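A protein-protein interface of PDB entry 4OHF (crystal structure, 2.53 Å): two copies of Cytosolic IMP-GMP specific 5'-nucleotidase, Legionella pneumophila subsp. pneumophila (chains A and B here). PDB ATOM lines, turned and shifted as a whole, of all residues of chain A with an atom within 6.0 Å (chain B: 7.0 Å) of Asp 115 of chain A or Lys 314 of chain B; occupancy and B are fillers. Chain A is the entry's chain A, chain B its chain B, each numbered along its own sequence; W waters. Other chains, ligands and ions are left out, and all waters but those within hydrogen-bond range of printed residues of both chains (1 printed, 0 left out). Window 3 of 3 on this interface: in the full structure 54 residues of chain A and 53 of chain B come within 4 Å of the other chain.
Of the printed residues of chain B, Arg 110 of chain A touches Asn 317.
Of the printed residues of chain B, Ser 111 of chain A touches Lys 313 (2.8 Å) and Lys 314 (3.0 Å).
Printed residues of chain B within 4 Å of Tyr 113 of chain A: Lys 313.
Asp 115 of chain A touches just these residues of chain B: Leu 310 (3.7 Å) and Lys 314 (3.9 Å).
Printed residues of chain A within 4 Å of Leu 310 of chain B: Asp 115.
Of the printed residues of chain A, Lys 313 of chain B touches Ser 111 and Tyr 113.
The nearest residue of chain B that does not touch Asp 115 of chain A is Arg 311 of chain B (6.7 Å).
Among the printed residues, merely in contact across the chains: Ser 111 of chain A with Lys 314 of chain B (3.0 Å), Arg 110 of chain A with Asn 317 of chain B (3.6 Å), Tyr 113 of chain A with Lys 313 of chain B (3.6 Å) and Asp 115 of chain A with Leu 310 of chain B (3.7 Å).
The side-chain hydroxyl (OG) of Ser 111 of chain A sits close to the backbone NH (N) of Tyr 113 of chain A (3.3 Å).
The backbone NH (N) of Gly 117 of chain A lies within hydrogen-bond range of the side-chain carboxylate (OD1) of Asp 115 of chain A (2.6 Å).
No position is printed for both chains.
Of the 6 pairs that touch across the chains among the printed residues, none has its exchanged pair printed and touching as well.
Water W1 bridges the side-chain amino group (NZ) of Lys 314 of chain B (2.8 Å) and the side-chain carboxylate (OD2) of Asp 115 of chain A (2.9 Å).
Of the 11 printed residues of chain A, 4 touch a printed residue of chain B.
Printed residues of chain A that touch a printed residue of chain B: Arg 110, Ser 111, Tyr 113 and Asp 115.
Of the 10 printed residues of chain B, 4 touch a printed residue of chain A.
Hydrophobic or aromatic side chains of chain B within 4 Å of the printed part of chain A: Leu 310.
Among the printed residues, Asp or Glu carboxylates within 4 Å of a Lys or Arg side-chain nitrogen of the other chain: Asp 115 of chain A with Lys 314 of chain B.
The side-chain hydroxyl (OG) of Ser 111 of chain A is in hydrogen-bond range of the backbone carbonyl oxygen (O) of Lys 313 of chain B (2.8 Å).
OD2 of Asp 115 of chain A is in salt-bridge range of NZ of Lys 314 of chain B (3.99 Å).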
ATOM      1  N   GLY A  88     -11.103  15.563  19.126  1.00  0.00           N
ATOM      2  CA  GLY A  88     -10.685  16.772  18.435  1.00  0.00           C
ATOM      3  C   GLY A  88      -9.997  17.817  19.286  1.00  0.00           C
ATOM      4  O   GLY A  88      -9.863  18.964  18.866  1.00  0.00           O
ATOM      5  N   ARG A 110      -9.098  29.702  20.009  1.00  0.00           N
ATOM      6  CA  ARG A 110     -10.075  30.102  21.020  1.00  0.00           C
ATOM      7  C   ARG A 110     -10.370  28.903  21.918  1.00  0.00           C
ATOM      8  O   ARG A 110     -10.189  28.955  23.141  1.00  0.00           O
ATOM      9  CB  ARG A 110     -11.369  30.584  20.342  1.00  0.00           C
ATOM     10  CG  ARG A 110     -11.965  31.871  20.948  1.00  0.00           C
ATOM     11  CD  ARG A 110     -10.940  33.023  20.961  1.00  0.00           C
ATOM     12  NE  ARG A 110     -10.420  33.334  19.627  1.00  0.00           N
ATOM     13  CZ  ARG A 110      -9.141  33.590  19.359  1.00  0.00           C
ATOM     14  NH1 ARG A 110      -8.237  33.573  20.331  1.00  0.00           N
ATOM     15  NH2 ARG A 110      -8.762  33.860  18.116  1.00  0.00           N
ATOM     16  N   SER A 111     -10.813  27.821  21.292  1.00  0.00           N
ATOM     17  CA  SER A 111     -11.126  26.591  21.999  1.00  0.00           C
ATOM     18  C   SER A 111      -9.993  25.605  21.759  1.00  0.00           C
ATOM     19  O   SER A 111      -9.212  25.776  20.832  1.00  0.00           O
ATOM     20  CB  SER A 111     -12.445  26.007  21.475  1.00  0.00           C
ATOM     21  OG  SER A 111     -12.780  24.813  22.156  1.00  0.00           O
ATOM     22  N   TYR A 113     -10.628  22.585  21.078  1.00  0.00           N
ATOM     23  CA  TYR A 113     -11.225  21.653  20.134  1.00  0.00           C
ATOM     24  C   TYR A 113     -11.269  22.254  18.737  1.00  0.00           C
ATOM     25  O   TYR A 113     -11.700  23.390  18.553  1.00  0.00           O
ATOM     26  CB  TYR A 113     -12.658  21.293  20.553  1.00  0.00           C
ATOM     27  CG  TYR A 113     -12.759  20.501  21.836  1.00  0.00           C
ATOM     28  CD1 TYR A 113     -12.796  21.137  23.075  1.00  0.00           C
ATOM     29  CD2 TYR A 113     -12.784  19.111  21.811  1.00  0.00           C
ATOM     30  CE1 TYR A 113     -12.851  20.405  24.254  1.00  0.00           C
ATOM     31  CE2 TYR A 113     -12.841  18.372  22.979  1.00  0.00           C
ATOM     32  CZ  TYR A 113     -12.872  19.018  24.199  1.00  0.00           C
ATOM     33  OH  TYR A 113     -12.915  18.266  25.359  1.00  0.00           O
ATOM     34  N   VAL A 114     -10.828  21.492  17.748  1.00  0.00           N
ATOM     35  CA  VAL A 114     -10.861  21.975  16.378  1.00  0.00           C
ATOM     36  C   VAL A 114     -11.958  21.224  15.645  1.00  0.00           C
ATOM     37  O   VAL A 114     -12.304  20.104  16.022  1.00  0.00           O
ATOM     38  CB  VAL A 114      -9.514  21.746  15.654  1.00  0.00           C
ATOM     39  CG1 VAL A 114      -8.421  22.553  16.335  1.00  0.00           C
ATOM     40  CG2 VAL A 114      -9.163  20.272  15.645  1.00  0.00           C
ATOM     41  N   ASP A 115     -12.517  21.848  14.612  1.00  0.00           N
ATOM     42  CA  ASP A 115     -13.570  21.229  13.811  1.00  0.00           C
ATOM     43  C   ASP A 115     -12.928  20.730  12.514  1.00  0.00           C
ATOM     44  O   ASP A 115     -12.595  21.523  11.635  1.00  0.00           O
ATOM     45  CB  ASP A 115     -14.660  22.258  13.481  1.00  0.00           C
ATOM     46  CG  ASP A 115     -15.849  21.643  12.755  1.00  0.00           C
ATOM     47  OD1 ASP A 115     -15.675  20.595  12.095  1.00  0.00           O
ATOM     48  OD2 ASP A 115     -16.961  22.218  12.832  1.00  0.00           O
ATOM     49  N   LEU A 116     -12.738  19.421  12.402  1.00  0.00           N
ATOM     50  CA  LEU A 116     -12.131  18.852  11.205  1.00  0.00           C
ATOM     51  C   LEU A 116     -13.094  18.926  10.023  1.00  0.00           C
ATOM     52  O   LEU A 116     -12.783  18.464   8.929  1.00  0.00           O
ATOM     53  CB  LEU A 116     -11.704  17.405  11.466  1.00  0.00           C
ATOM     54  CG  LEU A 116     -10.239  17.176  11.843  1.00  0.00           C
ATOM     55  CD1 LEU A 116      -9.711  18.315  12.700  1.00  0.00           C
ATOM     56  CD2 LEU A 116     -10.117  15.844  12.569  1.00  0.00           C
ATOM     57  N   GLY A 117     -14.270  19.503  10.255  1.00  0.00           N
ATOM     58  CA  GLY A 117     -15.239  19.655   9.183  1.00  0.00           C
ATOM     59  C   GLY A 117     -14.822  20.853   8.344  1.00  0.00           C
ATOM     60  O   GLY A 117     -15.188  20.985   7.169  1.00  0.00           O
ATOM     61  N   ASP A 118     -14.048  21.734   8.975  1.00  0.00           N
ATOM     62  CA  ASP A 118     -13.530  22.923   8.328  1.00  0.00           C
ATOM     63  C   ASP A 118     -12.430  22.450   7.394  1.00  0.00           C
ATOM     64  O   ASP A 118     -11.392  21.956   7.838  1.00  0.00           O
ATOM     65  CB  ASP A 118     -12.963  23.882   9.371  1.00  0.00           C
ATOM     66  CG  ASP A 118     -12.355  25.131   8.756  1.00  0.00           C
ATOM     67  OD1 ASP A 118     -11.956  26.027   9.534  1.00  0.00           O
ATOM     68  OD2 ASP A 118     -12.271  25.220   7.509  1.00  0.00           O
ATOM     69  N   PRO A 119     -12.648  22.589   6.078  1.00  0.00           N
ATOM     70  CA  PRO A 119     -11.686  22.178   5.049  1.00  0.00           C
ATOM     71  C   PRO A 119     -10.289  22.781   5.214  1.00  0.00           C
ATOM     72  O   PRO A 119      -9.356  22.415   4.502  1.00  0.00           O
ATOM     73  CB  PRO A 119     -12.369  22.607   3.752  1.00  0.00           C
ATOM     74  CG  PRO A 119     -13.217  23.776   4.183  1.00  0.00           C
ATOM     75  CD  PRO A 119     -13.802  23.279   5.474  1.00  0.00           C
ATOM     76  N   TYR A 121      -8.375  22.362   7.774  1.00  0.00           N
ATOM     77  CA  TYR A 121      -7.508  21.369   8.389  1.00  0.00           C
ATOM     78  C   TYR A 121      -7.275  20.211   7.422  1.00  0.00           C
ATOM     79  O   TYR A 121      -8.193  19.779   6.716  1.00  0.00           O
ATOM     80  CB  TYR A 121      -8.130  20.826   9.677  1.00  0.00           C
ATOM     81  CG  TYR A 121      -8.332  21.857  10.758  1.00  0.00           C
ATOM     82  CD1 TYR A 121      -9.574  22.472  10.937  1.00  0.00           C
ATOM     83  CD2 TYR A 121      -7.279  22.237  11.589  1.00  0.00           C
ATOM     84  CE1 TYR A 121      -9.757  23.438  11.914  1.00  0.00           C
ATOM     85  CE2 TYR A 121      -7.450  23.205  12.566  1.00  0.00           C
ATOM     86  CZ  TYR A 121      -8.693  23.800  12.722  1.00  0.00           C
ATOM     87  OH  TYR A 121      -8.879  24.760  13.684  1.00  0.00           O
ATOM     88  N   TYR B 252     -22.719  29.582  23.270  1.00  0.00           N
ATOM     89  CA  TYR B 252     -22.101  29.935  21.995  1.00  0.00           C
ATOM     90  C   TYR B 252     -22.651  31.143  21.252  1.00  0.00           C
ATOM     91  O   TYR B 252     -22.003  31.646  20.331  1.00  0.00           O
ATOM     92  CB  TYR B 252     -22.130  28.723  21.051  1.00  0.00           C
ATOM     93  CG  TYR B 252     -23.517  28.187  20.773  1.00  0.00           C
ATOM     94  CD1 TYR B 252     -23.956  26.991  21.356  1.00  0.00           C
ATOM     95  CD2 TYR B 252     -24.383  28.858  19.916  1.00  0.00           C
ATOM     96  CE1 TYR B 252     -25.221  26.477  21.086  1.00  0.00           C
ATOM     97  CE2 TYR B 252     -25.660  28.352  19.637  1.00  0.00           C
ATOM     98  CZ  TYR B 252     -26.067  27.159  20.228  1.00  0.00           C
ATOM     99  OH  TYR B 252     -27.315  26.654  19.965  1.00  0.00           O
ATOM    100  N   ILE B 309     -22.818  18.520  20.894  1.00  0.00           N
ATOM    101  CA  ILE B 309     -21.650  18.632  21.755  1.00  0.00           C
ATOM    102  C   ILE B 309     -20.507  19.379  21.075  1.00  0.00           C
ATOM    103  O   ILE B 309     -19.760  20.108  21.719  1.00  0.00           O
ATOM    104  CB  ILE B 309     -21.159  17.222  22.175  1.00  0.00           C
ATOM    105  CG1 ILE B 309     -22.340  16.396  22.701  1.00  0.00           C
ATOM    106  CG2 ILE B 309     -20.085  17.335  23.239  1.00  0.00           C
ATOM    107  CD1 ILE B 309     -21.972  14.987  23.148  1.00  0.00           C
ATOM    108  N   LEU B 310     -20.382  19.200  19.768  1.00  0.00           N
ATOM    109  CA  LEU B 310     -19.321  19.841  18.997  1.00  0.00           C
ATOM    110  C   LEU B 310     -19.451  21.363  18.925  1.00  0.00           C
ATOM    111  O   LEU B 310     -18.537  22.091  19.324  1.00  0.00           O
ATOM    112  CB  LEU B 310     -19.284  19.240  17.581  1.00  0.00           C
ATOM    113  CG  LEU B 310     -18.228  19.686  16.551  1.00  0.00           C
ATOM    114  CD1 LEU B 310     -18.718  20.935  15.800  1.00  0.00           C
ATOM    115  CD2 LEU B 310     -16.876  19.927  17.245  1.00  0.00           C
ATOM    116  N   ARG B 311     -20.583  21.840  18.416  1.00  0.00           N
ATOM    117  CA  ARG B 311     -20.814  23.275  18.298  1.00  0.00           C
ATOM    118  C   ARG B 311     -20.645  23.980  19.638  1.00  0.00           C
ATOM    119  O   ARG B 311     -20.205  25.127  19.692  1.00  0.00           O
ATOM    120  CB  ARG B 311     -22.218  23.532  17.743  1.00  0.00           C
ATOM    121  CG  ARG B 311     -22.671  24.974  17.811  1.00  0.00           C
ATOM    122  CD  ARG B 311     -23.954  25.166  17.013  1.00  0.00           C
ATOM    123  NE  ARG B 311     -24.438  26.548  17.019  1.00  0.00           N
ATOM    124  CZ  ARG B 311     -23.658  27.625  16.962  1.00  0.00           C
ATOM    125  NH1 ARG B 311     -22.337  27.501  16.903  1.00  0.00           N
ATOM    126  NH2 ARG B 311     -24.197  28.835  16.939  1.00  0.00           N
ATOM    127  N   LEU B 312     -20.981  23.280  20.718  1.00  0.00           N
ATOM    128  CA  LEU B 312     -20.880  23.838  22.057  1.00  0.00           C
ATOM    129  C   LEU B 312     -19.454  23.838  22.618  1.00  0.00           C
ATOM    130  O   LEU B 312     -19.000  24.847  23.151  1.00  0.00           O
ATOM    131  CB  LEU B 312     -21.814  23.081  22.995  1.00  0.00           C
ATOM    132  CG  LEU B 312     -22.168  23.770  24.312  1.00  0.00           C
ATOM    133  CD1 LEU B 312     -23.381  23.081  24.910  1.00  0.00           C
ATOM    134  CD2 LEU B 312     -20.983  23.732  25.269  1.00  0.00           C
ATOM    135  N   LYS B 313     -18.751  22.716  22.512  1.00  0.00           N
ATOM    136  CA  LYS B 313     -17.386  22.652  23.021  1.00  0.00           C
ATOM    137  C   LYS B 313     -16.442  23.413  22.090  1.00  0.00           C
ATOM    138  O   LYS B 313     -15.305  23.705  22.455  1.00  0.00           O
ATOM    139  CB  LYS B 313     -16.910  21.193  23.159  1.00  0.00           C
ATOM    140  CG  LYS B 313     -17.772  20.309  24.056  1.00  0.00           C
ATOM    141  CD  LYS B 313     -17.718  20.703  25.528  1.00  0.00           C
ATOM    142  CE  LYS B 313     -16.409  20.300  26.166  1.00  0.00           C
ATOM    143  NZ  LYS B 313     -16.292  20.839  27.548  1.00  0.00           N
ATOM    144  N   LYS B 314     -16.916  23.744  20.894  1.00  0.00           N
ATOM    145  CA  LYS B 314     -16.094  24.462  19.919  1.00  0.00           C
ATOM    146  C   LYS B 314     -16.065  25.974  20.143  1.00  0.00           C
ATOM    147  O   LYS B 314     -15.025  26.611  19.999  1.00  0.00           O
ATOM    148  CB  LYS B 314     -16.594  24.184  18.498  1.00  0.00           C
ATOM    149  CG  LYS B 314     -15.747  24.830  17.411  1.00  0.00           C
ATOM    150  CD  LYS B 314     -16.386  24.735  16.026  1.00  0.00           C
ATOM    151  CE  LYS B 314     -17.557  25.704  15.871  1.00  0.00           C
ATOM    152  NZ  LYS B 314     -18.193  25.615  14.520  1.00  0.00           N
ATOM    153  N   ASP B 315     -17.207  26.545  20.500  1.00  0.00           N
ATOM    154  CA  ASP B 315     -17.287  27.986  20.699  1.00  0.00           C
ATOM    155  C   ASP B 315     -17.311  28.427  22.147  1.00  0.00           C
ATOM    156  O   ASP B 315     -17.481  29.610  22.421  1.00  0.00           O
ATOM    157  CB  ASP B 315     -18.535  28.539  20.015  1.00  0.00           C
ATOM    158  CG  ASP B 315     -18.596  28.198  18.547  1.00  0.00           C
ATOM    159  OD1 ASP B 315     -19.704  28.292  17.973  1.00  0.00           O
ATOM    160  OD2 ASP B 315     -17.542  27.847  17.970  1.00  0.00           O
ATOM    161  N   CYS B 316     -17.160  27.500  23.085  1.00  0.00           N
ATOM    162  CA  CYS B 316     -17.194  27.900  24.476  1.00  0.00           C
ATOM    163  C   CYS B 316     -15.816  27.885  25.120  1.00  0.00           C
ATOM    164  O   CYS B 316     -15.208  28.943  25.308  1.00  0.00           O
ATOM    165  CB  CYS B 316     -18.147  27.016  25.266  1.00  0.00           C
ATOM    166  SG  CYS B 316     -18.493  27.670  26.904  1.00  0.00           S
ATOM    167  N   ASN B 317     -15.347  26.691  25.461  1.00  0.00           N
ATOM    168  CA  ASN B 317     -14.036  26.452  26.078  1.00  0.00           C
ATOM    169  C   ASN B 317     -14.027  26.349  27.606  1.00  0.00           C
ATOM    170  O   ASN B 317     -12.965  26.269  28.233  1.00  0.00           O
ATOM    171  CB  ASN B 317     -12.961  27.451  25.575  1.00  0.00           C
ATOM    172  CG  ASN B 317     -12.824  28.690  26.446  1.00  0.00           C
ATOM    173  OD1 ASN B 317     -11.867  29.452  26.300  1.00  0.00           O
ATOM    174  ND2 ASN B 317     -13.775  28.908  27.345  1.00  0.00           N
HETATM  175  O   HOH W   1     -16.528  25.056  12.382  1.00  0.00           O
